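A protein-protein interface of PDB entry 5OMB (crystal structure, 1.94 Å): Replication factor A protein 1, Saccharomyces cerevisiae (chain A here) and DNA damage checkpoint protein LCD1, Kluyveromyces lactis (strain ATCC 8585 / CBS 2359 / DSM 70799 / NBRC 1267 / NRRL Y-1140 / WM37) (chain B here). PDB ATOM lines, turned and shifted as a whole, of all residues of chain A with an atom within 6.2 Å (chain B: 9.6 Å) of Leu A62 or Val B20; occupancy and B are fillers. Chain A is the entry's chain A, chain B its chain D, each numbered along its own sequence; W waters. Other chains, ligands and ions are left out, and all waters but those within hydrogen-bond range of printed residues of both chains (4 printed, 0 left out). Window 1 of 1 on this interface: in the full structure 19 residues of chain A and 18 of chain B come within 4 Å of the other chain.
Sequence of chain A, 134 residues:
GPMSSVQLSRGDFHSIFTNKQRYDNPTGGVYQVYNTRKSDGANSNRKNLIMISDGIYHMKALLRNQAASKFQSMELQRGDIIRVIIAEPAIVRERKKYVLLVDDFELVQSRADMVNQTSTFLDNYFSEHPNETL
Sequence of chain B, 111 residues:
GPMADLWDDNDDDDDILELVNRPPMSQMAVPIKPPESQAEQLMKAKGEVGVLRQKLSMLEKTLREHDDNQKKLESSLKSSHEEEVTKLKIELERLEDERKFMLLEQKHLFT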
ATOM      1  N   ASN A  45     -28.875  24.059 -22.748  1.00  0.00           N
ATOM      2  CA  ASN A  45     -27.453  24.457 -22.778  1.00  0.00           C
ATOM      3  C   ASN A  45     -26.563  23.373 -23.402  1.00  0.00           C
ATOM      4  O   ASN A  45     -25.632  23.706 -24.149  1.00  0.00           O
ATOM      5  CB  ASN A  45     -26.917  24.822 -21.375  1.00  0.00           C
ATOM      6  CG  ASN A  45     -25.849  25.898 -21.392  1.00  0.00           C
ATOM      7  OD1 ASN A  45     -25.899  26.870 -22.170  1.00  0.00           O
ATOM      8  ND2 ASN A  45     -24.870  25.762 -20.507  1.00  0.00           N
ATOM      9  N   ASN A  48     -25.995  23.059 -27.276  1.00  0.00           N
ATOM     10  CA  ASN A  48     -24.997  23.921 -27.906  1.00  0.00           C
ATOM     11  C   ASN A  48     -23.673  23.197 -28.071  1.00  0.00           C
ATOM     12  O   ASN A  48     -22.814  23.653 -28.816  1.00  0.00           O
ATOM     13  CB  ASN A  48     -24.811  25.190 -27.094  1.00  0.00           C
ATOM     14  CG  ASN A  48     -25.994  26.135 -27.146  1.00  0.00           C
ATOM     15  OD1 ASN A  48     -26.952  25.960 -27.921  1.00  0.00           O
ATOM     16  ND2 ASN A  48     -25.917  27.195 -26.354  1.00  0.00           N
ATOM     17  N   LEU A  49     -23.511  22.054 -27.389  1.00  0.00           N
ATOM     18  CA  LEU A  49     -22.289  21.283 -27.498  1.00  0.00           C
ATOM     19  C   LEU A  49     -22.474  20.219 -28.542  1.00  0.00           C
ATOM     20  O   LEU A  49     -23.229  19.272 -28.350  1.00  0.00           O
ATOM     21  CB  LEU A  49     -21.838  20.708 -26.151  1.00  0.00           C
ATOM     22  CG  LEU A  49     -20.517  19.945 -26.169  1.00  0.00           C
ATOM     23  CD1 LEU A  49     -19.372  20.839 -26.582  1.00  0.00           C
ATOM     24  CD2 LEU A  49     -20.246  19.325 -24.828  1.00  0.00           C
ATOM     25  N   ILE A  50     -21.811  20.412 -29.674  1.00  0.00           N
ATOM     26  CA  ILE A  50     -21.900  19.510 -30.800  1.00  0.00           C
ATOM     27  C   ILE A  50     -20.553  18.886 -31.134  1.00  0.00           C
ATOM     28  O   ILE A  50     -19.514  19.285 -30.613  1.00  0.00           O
ATOM     29  CB  ILE A  50     -22.550  20.234 -32.027  1.00  0.00           C
ATOM     30  CG1 ILE A  50     -21.595  21.288 -32.653  1.00  0.00           C
ATOM     31  CG2 ILE A  50     -23.927  20.832 -31.673  1.00  0.00           C
ATOM     32  CD1 ILE A  50     -21.975  21.783 -34.068  1.00  0.00           C
ATOM     33  N   LYS A  60     -15.125  18.582 -30.345  1.00  0.00           N
ATOM     34  CA  LYS A  60     -16.272  19.250 -29.762  1.00  0.00           C
ATOM     35  C   LYS A  60     -16.274  20.708 -30.169  1.00  0.00           C
ATOM     36  O   LYS A  60     -15.220  21.328 -30.305  1.00  0.00           O
ATOM     37  CB  LYS A  60     -16.299  19.102 -28.235  1.00  0.00           C
ATOM     38  CG  LYS A  60     -16.466  17.656 -27.773  1.00  0.00           C
ATOM     39  CD  LYS A  60     -16.716  17.568 -26.279  1.00  0.00           C
ATOM     40  CE  LYS A  60     -16.846  16.135 -25.796  1.00  0.00           C
ATOM     41  NZ  LYS A  60     -18.102  15.494 -26.279  1.00  0.00           N
ATOM     42  N   ALA A  61     -17.459  21.247 -30.412  1.00  0.00           N
ATOM     43  CA  ALA A  61     -17.604  22.668 -30.719  1.00  0.00           C
ATOM     44  C   ALA A  61     -18.707  23.172 -29.825  1.00  0.00           C
ATOM     45  O   ALA A  61     -19.767  22.537 -29.733  1.00  0.00           O
ATOM     46  CB  ALA A  61     -17.975  22.889 -32.186  1.00  0.00           C
ATOM     47  N   LEU A  62     -18.462  24.290 -29.149  1.00  0.00           N
ATOM     48  CA  LEU A  62     -19.495  24.903 -28.315  1.00  0.00           C
ATOM     49  C   LEU A  62     -20.043  26.115 -29.054  1.00  0.00           C
ATOM     50  O   LEU A  62     -19.320  27.089 -29.279  1.00  0.00           O
ATOM     51  CB  LEU A  62     -18.982  25.315 -26.907  1.00  0.00           C
ATOM     52  CG  LEU A  62     -20.033  26.008 -25.994  1.00  0.00           C
ATOM     53  CD1 LEU A  62     -21.079  25.013 -25.485  1.00  0.00           C
ATOM     54  CD2 LEU A  62     -19.362  26.786 -24.847  1.00  0.00           C
ATOM     55  N   LEU A  63     -21.307  26.042 -29.438  1.00  0.00           N
ATOM     56  CA  LEU A  63     -21.998  27.138 -30.109  1.00  0.00           C
ATOM     57  C   LEU A  63     -22.400  28.147 -29.070  1.00  0.00           C
ATOM     58  O   LEU A  63     -22.958  27.782 -28.031  1.00  0.00           O
ATOM     59  CB  LEU A  63     -23.266  26.642 -30.836  1.00  0.00           C
ATOM     60  CG  LEU A  63     -23.048  25.627 -31.935  1.00  0.00           C
ATOM     61  CD1 LEU A  63     -24.276  24.733 -32.086  1.00  0.00           C
ATOM     62  CD2 LEU A  63     -22.692  26.304 -33.242  1.00  0.00           C
ATOM     63  N   ARG A  64     -22.118  29.426 -29.341  1.00  0.00           N
ATOM     64  CA  ARG A  64     -22.474  30.497 -28.415  1.00  0.00           C
ATOM     65  C   ARG A  64     -23.041  31.660 -29.222  1.00  0.00           C
ATOM     66  O   ARG A  64     -22.926  31.679 -30.445  1.00  0.00           O
ATOM     67  CB  ARG A  64     -21.225  30.989 -27.641  1.00  0.00           C
ATOM     68  CG  ARG A  64     -20.270  29.929 -27.144  1.00  0.00           C
ATOM     69  CD  ARG A  64     -19.185  30.537 -26.289  1.00  0.00           C
ATOM     70  NE  ARG A  64     -18.427  31.566 -27.001  1.00  0.00           N
ATOM     71  CZ  ARG A  64     -17.469  32.296 -26.442  1.00  0.00           C
ATOM     72  NH1 ARG A  64     -17.152  32.124 -25.168  1.00  0.00           N
ATOM     73  NH2 ARG A  64     -16.813  33.199 -27.158  1.00  0.00           N
ATOM     74  N   ASN A  65     -23.642  32.630 -28.544  1.00  0.00           N
ATOM     75  CA  ASN A  65     -24.086  33.883 -29.162  1.00  0.00           C
ATOM     76  C   ASN A  65     -24.960  33.680 -30.423  1.00  0.00           C
ATOM     77  O   ASN A  65     -25.865  32.840 -30.374  1.00  0.00           O
ATOM     78  CB  ASN A  65     -22.836  34.772 -29.420  1.00  0.00           C
ATOM     79  CG  ASN A  65     -22.149  35.123 -28.142  1.00  0.00           C
ATOM     80  OD1 ASN A  65     -22.746  35.761 -27.298  1.00  0.00           O
ATOM     81  ND2 ASN A  65     -20.936  34.618 -27.919  1.00  0.00           N
ATOM     82  N   ALA A  68     -25.290  29.983 -31.680  1.00  0.00           N
ATOM     83  CA  ALA A  68     -26.201  29.068 -30.952  1.00  0.00           C
ATOM     84  C   ALA A  68     -27.647  29.284 -31.407  1.00  0.00           C
ATOM     85  O   ALA A  68     -28.381  28.311 -31.619  1.00  0.00           O
ATOM     86  CB  ALA A  68     -26.096  29.283 -29.452  1.00  0.00           C
ATOM     87  N   VAL A  99     -11.822  22.209 -27.320  1.00  0.00           N
ATOM     88  CA  VAL A  99     -13.107  22.711 -27.811  1.00  0.00           C
ATOM     89  C   VAL A  99     -12.905  23.940 -28.707  1.00  0.00           C
ATOM     90  O   VAL A  99     -11.963  24.713 -28.509  1.00  0.00           O
ATOM     91  CB  VAL A  99     -14.150  22.947 -26.666  1.00  0.00           C
ATOM     92  CG1 VAL A  99     -13.661  23.978 -25.651  1.00  0.00           C
ATOM     93  CG2 VAL A  99     -15.541  23.319 -27.213  1.00  0.00           C
ATOM     94  N   LEU A 100     -13.768  24.069 -29.723  1.00  0.00           N
ATOM     95  CA  LEU A 100     -13.815  25.227 -30.589  1.00  0.00           C
ATOM     96  C   LEU A 100     -15.068  25.986 -30.199  1.00  0.00           C
ATOM     97  O   LEU A 100     -16.175  25.455 -30.308  1.00  0.00           O
ATOM     98  CB  LEU A 100     -13.852  24.860 -32.074  1.00  0.00           C
ATOM     99  CG  LEU A 100     -13.745  26.045 -33.063  1.00  0.00           C
ATOM    100  CD1 LEU A 100     -12.376  26.726 -32.973  1.00  0.00           C
ATOM    101  CD2 LEU A 100     -14.006  25.570 -34.487  1.00  0.00           C
ATOM    102  N   LEU A 101     -14.885  27.186 -29.653  1.00  0.00           N
ATOM    103  CA  LEU A 101     -16.005  28.044 -29.243  1.00  0.00           C
ATOM    104  C   LEU A 101     -16.438  28.809 -30.498  1.00  0.00           C
ATOM    105  O   LEU A 101     -15.664  29.608 -31.008  1.00  0.00           O
ATOM    106  CB  LEU A 101     -15.556  29.006 -28.155  1.00  0.00           C
ATOM    107  CG  LEU A 101     -14.868  28.367 -26.919  1.00  0.00           C
ATOM    108  CD1 LEU A 101     -14.538  29.432 -25.912  1.00  0.00           C
ATOM    109  CD2 LEU A 101     -15.727  27.263 -26.308  1.00  0.00           C
ATOM    110  N   VAL A 102     -17.618  28.475 -31.050  1.00  0.00           N
ATOM    111  CA  VAL A 102     -18.103  29.053 -32.306  1.00  0.00           C
ATOM    112  C   VAL A 102     -19.162  30.121 -32.011  1.00  0.00           C
ATOM    113  O   VAL A 102     -20.214  29.805 -31.457  1.00  0.00           O
ATOM    114  CB  VAL A 102     -18.612  27.957 -33.281  1.00  0.00           C
ATOM    115  CG1 VAL A 102     -19.178  28.571 -34.575  1.00  0.00           C
ATOM    116  CG2 VAL A 102     -17.510  26.959 -33.605  1.00  0.00           C
ATOM    117  N   ASP A 103     -18.852  31.390 -32.353  1.00  0.00           N
ATOM    118  CA  ASP A 103     -19.741  32.534 -32.147  1.00  0.00           C
ATOM    119  C   ASP A 103     -20.581  32.887 -33.358  1.00  0.00           C
ATOM    120  O   ASP A 103     -21.610  33.548 -33.214  1.00  0.00           O
ATOM    121  CB  ASP A 103     -18.947  33.762 -31.646  1.00  0.00           C
ATOM    122  CG  ASP A 103     -18.396  33.521 -30.249  1.00  0.00           C
ATOM    123  OD1 ASP A 103     -19.156  33.012 -29.395  1.00  0.00           O
ATOM    124  OD2 ASP A 103     -17.180  33.801 -30.022  1.00  0.00           O
ATOM    125  N   ASP B  13     -19.405  17.382 -19.181  1.00  0.00           N
ATOM    126  CA  ASP B  13     -18.791  18.387 -20.051  1.00  0.00           C
ATOM    127  C   ASP B  13     -19.059  19.803 -19.507  1.00  0.00           C
ATOM    128  O   ASP B  13     -19.050  20.772 -20.276  1.00  0.00           O
ATOM    129  CB  ASP B  13     -19.329  18.248 -21.490  1.00  0.00           C
ATOM    130  CG  ASP B  13     -18.565  17.271 -22.362  1.00  0.00           C
ATOM    131  OD1 ASP B  13     -17.325  17.393 -22.444  1.00  0.00           O
ATOM    132  OD2 ASP B  13     -19.210  16.421 -23.003  1.00  0.00           O
ATOM    133  N   ASP B  14     -19.273  19.922 -18.176  1.00  0.00           N
ATOM    134  CA  ASP B  14     -19.580  21.192 -17.512  1.00  0.00           C
ATOM    135  C   ASP B  14     -18.456  22.208 -17.586  1.00  0.00           C
ATOM    136  O   ASP B  14     -18.733  23.409 -17.570  1.00  0.00           O
ATOM    137  CB  ASP B  14     -20.046  20.982 -16.065  1.00  0.00           C
ATOM    138  CG  ASP B  14     -21.544  20.745 -15.991  1.00  0.00           C
ATOM    139  OD1 ASP B  14     -21.953  19.562 -15.907  1.00  0.00           O
ATOM    140  OD2 ASP B  14     -22.314  21.742 -16.083  1.00  0.00           O
ATOM    141  N   ASP B  15     -17.192  21.733 -17.697  1.00  0.00           N
ATOM    142  CA  ASP B  15     -16.012  22.599 -17.862  1.00  0.00           C
ATOM    143  C   ASP B  15     -16.033  23.277 -19.259  1.00  0.00           C
ATOM    144  O   ASP B  15     -15.467  24.350 -19.441  1.00  0.00           O
ATOM    145  CB  ASP B  15     -14.694  21.836 -17.611  1.00  0.00           C
ATOM    146  CG  ASP B  15     -14.593  20.419 -18.164  1.00  0.00           C
ATOM    147  OD1 ASP B  15     -15.472  20.018 -18.956  1.00  0.00           O
ATOM    148  OD2 ASP B  15     -13.619  19.721 -17.821  1.00  0.00           O
ATOM    149  N   ILE B  16     -16.699  22.646 -20.227  1.00  0.00           N
ATOM    150  CA  ILE B  16     -16.854  23.202 -21.569  1.00  0.00           C
ATOM    151  C   ILE B  16     -18.063  24.157 -21.571  1.00  0.00           C
ATOM    152  O   ILE B  16     -17.934  25.301 -22.002  1.00  0.00           O
ATOM    153  CB  ILE B  16     -16.936  22.094 -22.654  1.00  0.00           C
ATOM    154  CG1 ILE B  16     -15.586  21.322 -22.749  1.00  0.00           C
ATOM    155  CG2 ILE B  16     -17.346  22.692 -24.018  1.00  0.00           C
ATOM    156  CD1 ILE B  16     -15.582  20.097 -23.677  1.00  0.00           C
ATOM    157  N   LEU B  17     -19.208  23.700 -21.022  1.00  0.00           N
ATOM    158  CA  LEU B  17     -20.479  24.440 -20.975  1.00  0.00           C
ATOM    159  C   LEU B  17     -20.407  25.750 -20.200  1.00  0.00           C
ATOM    160  O   LEU B  17     -21.140  26.686 -20.522  1.00  0.00           O
ATOM    161  CB  LEU B  17     -21.627  23.553 -20.463  1.00  0.00           C
ATOM    162  CG  LEU B  17     -21.944  22.327 -21.337  1.00  0.00           C
ATOM    163  CD1 LEU B  17     -22.733  21.287 -20.568  1.00  0.00           C
ATOM    164  CD2 LEU B  17     -22.642  22.715 -22.639  1.00  0.00           C
ATOM    165  N   GLU B  18     -19.488  25.852 -19.237  1.00  0.00           N
ATOM    166  CA  GLU B  18     -19.269  27.076 -18.456  1.00  0.00           C
ATOM    167  C   GLU B  18     -18.642  28.208 -19.310  1.00  0.00           C
ATOM    168  O   GLU B  18     -18.587  29.347 -18.859  1.00  0.00           O
ATOM    169  CB  GLU B  18     -18.426  26.783 -17.194  1.00  0.00           C
ATOM    170  CG  GLU B  18     -16.997  26.367 -17.502  1.00  0.00           C
ATOM    171  CD  GLU B  18     -16.028  26.196 -16.349  1.00  0.00           C
ATOM    172  OE1 GLU B  18     -16.455  26.308 -15.176  1.00  0.00           O
ATOM    173  OE2 GLU B  18     -14.835  25.931 -16.625  1.00  0.00           O
ATOM    174  N   LEU B  19     -18.172  27.888 -20.534  1.00  0.00           N
ATOM    175  CA  LEU B  19     -17.597  28.879 -21.460  1.00  0.00           C
ATOM    176  C   LEU B  19     -18.667  29.581 -22.315  1.00  0.00           C
ATOM    177  O   LEU B  19     -18.329  30.526 -23.018  1.00  0.00           O
ATOM    178  CB  LEU B  19     -16.529  28.241 -22.373  1.00  0.00           C
ATOM    179  CG  LEU B  19     -15.355  27.510 -21.691  1.00  0.00           C
ATOM    180  CD1 LEU B  19     -14.638  26.619 -22.676  1.00  0.00           C
ATOM    181  CD2 LEU B  19     -14.390  28.494 -21.034  1.00  0.00           C
ATOM    182  N   VAL B  20     -19.949  29.126 -22.255  1.00  0.00           N
ATOM    183  CA  VAL B  20     -21.063  29.691 -23.046  1.00  0.00           C
ATOM    184  C   VAL B  20     -21.245  31.208 -22.779  1.00  0.00           C
ATOM    185  O   VAL B  20     -21.453  31.969 -23.733  1.00  0.00           O
ATOM    186  CB  VAL B  20     -22.405  28.889 -22.938  1.00  0.00           C
ATOM    187  CG1 VAL B  20     -23.093  29.081 -21.585  1.00  0.00           C
ATOM    188  CG2 VAL B  20     -23.362  29.251 -24.071  1.00  0.00           C
ATOM    189  N   ASN B  21     -21.141  31.644 -21.516  1.00  0.00           N
ATOM    190  CA  ASN B  21     -21.285  33.075 -21.225  1.00  0.00           C
ATOM    191  C   ASN B  21     -19.935  33.766 -21.025  1.00  0.00           C
ATOM    192  O   ASN B  21     -19.924  34.952 -20.660  1.00  0.00           O
ATOM    193  CB  ASN B  21     -22.210  33.354 -20.017  1.00  0.00           C
ATOM    194  CG  ASN B  21     -23.476  32.530 -19.976  1.00  0.00           C
ATOM    195  OD1 ASN B  21     -24.364  32.659 -20.828  1.00  0.00           O
ATOM    196  ND2 ASN B  21     -23.591  31.686 -18.954  1.00  0.00           N
ATOM    197  N   ARG B  22     -18.794  33.039 -21.242  1.00  0.00           N
ATOM    198  CA  ARG B  22     -17.472  33.664 -21.079  1.00  0.00           C
ATOM    199  C   ARG B  22     -17.386  34.848 -22.064  1.00  0.00           C
ATOM    200  O   ARG B  22     -17.785  34.681 -23.225  1.00  0.00           O
ATOM    201  CB  ARG B  22     -16.312  32.655 -21.262  1.00  0.00           C
ATOM    202  CG  ARG B  22     -14.932  33.269 -20.971  1.00  0.00           C
ATOM    203  CD  ARG B  22     -13.809  32.281 -21.124  1.00  0.00           C
ATOM    204  NE  ARG B  22     -13.396  32.116 -22.518  1.00  0.00           N
ATOM    205  CZ  ARG B  22     -12.416  31.308 -22.902  1.00  0.00           C
ATOM    206  NH1 ARG B  22     -11.744  30.597 -22.010  1.00  0.00           N
ATOM    207  NH2 ARG B  22     -12.091  31.217 -24.179  1.00  0.00           N
ATOM    208  N   PRO B  23     -17.015  36.072 -21.602  1.00  0.00           N
ATOM    209  CA  PRO B  23     -16.987  37.230 -22.522  1.00  0.00           C
ATOM    210  C   PRO B  23     -16.206  36.935 -23.807  1.00  0.00           C
ATOM    211  O   PRO B  23     -15.109  36.385 -23.753  1.00  0.00           O
ATOM    212  CB  PRO B  23     -16.347  38.343 -21.679  1.00  0.00           C
ATOM    213  CG  PRO B  23     -16.646  37.952 -20.276  1.00  0.00           C
ATOM    214  CD  PRO B  23     -16.574  36.464 -20.239  1.00  0.00           C
ATOM    215  N   PRO B  24     -16.797  37.165 -24.989  1.00  0.00           N
ATOM    216  CA  PRO B  24     -16.098  36.776 -26.222  1.00  0.00           C
ATOM    217  C   PRO B  24     -14.941  37.700 -26.594  1.00  0.00           C
ATOM    218  O   PRO B  24     -14.933  38.869 -26.209  1.00  0.00           O
ATOM    219  CB  PRO B  24     -17.225  36.783 -27.258  1.00  0.00           C
ATOM    220  CG  PRO B  24     -18.162  37.824 -26.764  1.00  0.00           C
ATOM    221  CD  PRO B  24     -18.141  37.720 -25.277  1.00  0.00           C
ATOM    222  N   ALA B  29     -19.533  39.228 -31.616  1.00  0.00           N
ATOM    223  CA  ALA B  29     -20.237  38.076 -31.052  1.00  0.00           C
ATOM    224  C   ALA B  29     -21.285  38.656 -30.097  1.00  0.00           C
ATOM    225  O   ALA B  29     -20.927  39.299 -29.103  1.00  0.00           O
ATOM    226  CB  ALA B  29     -19.260  37.161 -30.316  1.00  0.00           C
ATOM    227  N   VAL B  30     -22.579  38.515 -30.452  1.00  0.00           N
ATOM    228  CA  VAL B  30     -23.691  39.102 -29.694  1.00  0.00           C
ATOM    229  C   VAL B  30     -24.523  38.074 -28.942  1.00  0.00           C
ATOM    230  O   VAL B  30     -24.961  37.109 -29.546  1.00  0.00           O
ATOM    231  CB  VAL B  30     -24.604  40.025 -30.561  1.00  0.00           C
ATOM    232  CG1 VAL B  30     -24.014  41.406 -30.677  1.00  0.00           C
ATOM    233  CG2 VAL B  30     -24.875  39.440 -31.938  1.00  0.00           C
ATOM    234  N   PRO B  31     -24.827  38.292 -27.642  1.00  0.00           N
ATOM    235  CA  PRO B  31     -25.630  37.295 -26.916  1.00  0.00           C
ATOM    236  C   PRO B  31     -27.106  37.328 -27.296  1.00  0.00           C
ATOM    237  O   PRO B  31     -27.702  38.392 -27.420  1.00  0.00           O
ATOM    238  CB  PRO B  31     -25.355  37.603 -25.435  1.00  0.00           C
ATOM    239  CG  PRO B  31     -24.905  38.981 -25.408  1.00  0.00           C
ATOM    240  CD  PRO B  31     -24.405  39.395 -26.757  1.00  0.00           C
ATOM    241  N   ILE B  32     -27.659  36.163 -27.609  1.00  0.00           N
ATOM    242  CA  ILE B  32     -29.072  36.066 -27.981  1.00  0.00           C
ATOM    243  C   ILE B  32     -29.695  35.052 -27.047  1.00  0.00           C
ATOM    244  O   ILE B  32     -29.341  33.877 -27.092  1.00  0.00           O
ATOM    245  CB  ILE B  32     -29.304  35.756 -29.493  1.00  0.00           C
ATOM    246  CG1 ILE B  32     -28.602  36.817 -30.364  1.00  0.00           C
ATOM    247  CG2 ILE B  32     -30.828  35.682 -29.813  1.00  0.00           C
ATOM    248  CD1 ILE B  32     -28.447  36.524 -31.766  1.00  0.00           C
ATOM    249  N   PRO B  34     -32.319  32.332 -25.442  1.00  0.00           N
ATOM    250  CA  PRO B  34     -33.137  31.324 -26.147  1.00  0.00           C
ATOM    251  C   PRO B  34     -34.570  31.793 -26.438  1.00  0.00           C
ATOM    252  O   PRO B  34     -35.067  32.673 -25.718  1.00  0.00           O
ATOM    253  CB  PRO B  34     -33.107  30.111 -25.208  1.00  0.00           C
ATOM    254  CG  PRO B  34     -31.877  30.282 -24.413  1.00  0.00           C
ATOM    255  CD  PRO B  34     -31.785  31.773 -24.181  1.00  0.00           C
HETATM  256  O   HOH W   1     -24.240  32.407 -25.592  1.00  0.00           O
HETATM  257  O   HOH W   2     -27.218  32.528 -28.079  1.00  0.00           O
HETATM  258  O   HOH W   3     -19.909  34.188 -24.896  1.00  0.00           O
HETATM  259  O   HOH W   4     -14.557  33.873 -24.658  1.00  0.00           O
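The side-chain carboxylate (OD2) of Asp B13 lies within salt-bridge range of the side-chain amino group (NZ) of Lys A60, 3.6 Å away. The backbone carbonyl oxygen of Leu B19 is in hydrogen-bond range of the guanidinium group of Arg A64, 2.9 Å away. NH1 of Arg A64 is in hydrogen-bond range of O of Arg B22, at 3.3 Å. The side-chain amide oxygen of Asn A65 sits close to the backbone carbonyl oxygen of Val B30 (3.4 Å). OD1 of Asn A65 sits close to N of Pro B31, at 3.3 Å.
The backbone carbonyl oxygen (O) of Asn A48 lies within hydrogen-bond range of the backbone NH (N) of Leu A63 (2.9 Å). O of Lys A60 is in hydrogen-bond range of N of Leu A100 (3.2 Å). The backbone carbonyl oxygen of Leu A62 lies within hydrogen-bond range of the backbone NH of Val A102 (2.8 Å). The backbone NH (N) of Arg A64 is in hydrogen-bond range of the backbone carbonyl oxygen (O) of Val A102 (2.9 Å). OD1 of Asp A103 lies within salt-bridge range of NE of Arg A64, at 2.9 Å. The side-chain amide nitrogen (ND2) of Asn A65 sits at hydrogen-bond distance from the side-chain carboxylate (OD1) of Asp A103 (2.8 Å).
Among the printed residues, pairs that only touch across the chains: Asn A45 with Leu B17, Asn A45 with Val B20, Asn A48 with Val B20, Leu A49 with Asp B13, Leu A49 with Ile B16, Lys A60 with Ile B16, Leu A62 with Ile B16, Leu A62 with Leu B17, Leu A62 with Leu B19, Leu A62 with Val B20, Arg A64 with Val B20, Arg A64 with Pro B24, Asn A65 with Ala B29, Val A99 with Ile B16, Leu A101 with Leu B19, Leu A101 with Arg B22 and Asp A103 with Ala B29.
No residue of chain B comes within 4 Å of Ala A61. No residue of chain B comes within 4 Å of Leu A63. Of the printed residues of chain B, Asn A65 touches Ala B29 (3.9 Å), Val B30 (3.2 Å) and Pro B31 (3.3 Å). Printed residues of chain B within 4 Å of Val A99: Ile B16. No residue of chain B comes within 4 Å of Val A102. Asp B15 touches none of the printed residues of chain A. Printed residues of chain A within 4 Å of Ile B16: Leu A49, Lys A60, Leu A62 and Val A99. Of the printed residues of chain A, Leu B19 touches Leu A62, Arg A64 and Leu A101. Of the printed residues of chain A, Val B20 touches Asn A45 (3.6 Å), Asn A48 (3.996 Å), Leu A62 (3.5 Å) and Arg A64 (3.7 Å). The nearest printed residue of chain A that does not touch Val B20 is Leu A63 (4.2 Å). The nearest printed residue of chain A that does not touch Pro B31 is Arg A64 (6.6 Å).
Printed residues of chain B that touch a printed residue of chain A: Asp B13, Ile B16, Leu B17, Leu B19, Val B20, Arg B22, Pro B24, Ala B29, Val B30 and Pro B31. Hydrophobic or aromatic side chains of chain B that line the printed part of chain A: Ile B16, Leu B17, Leu B19, Val B20, Pro B24, Ala B29 and Pro B31. Of the 16 printed residues of chain A, 10 touch a printed residue of chain B. Hydrophobic or aromatic side chains of chain A within 4 Å of the printed part of chain B: Leu A49, Leu A62, Val A99 and Leu A101. Among the printed residues, 22 pairs touch across the chains. Among the printed residues, Asp or Glu carboxylates within 4 Å of a Lys or Arg side-chain nitrogen of the other chain: Lys A60 with Asp B13 (3.6 Å).
Water W2 bridges O of Asn A65 (2.7 Å) and O of Ile B32 (2.7 Å). Water W4 lies within hydrogen-bond range of the backbone carbonyl oxygen of Pro B23 (2.7 Å), the guanidinium group of Arg B22 (3.0 Å) and the guanidinium group of Arg A64 (3.2 Å). Water W3 lies within hydrogen-bond range of O of Arg B22, O of Val B20, ND2 of Asn A65 and NH1 of Arg A64. Water W1 lies within hydrogen-bond range of the backbone NH of Asn A65 (3.0 Å) and the backbone carbonyl oxygen of Val B20 (3.4 Å).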
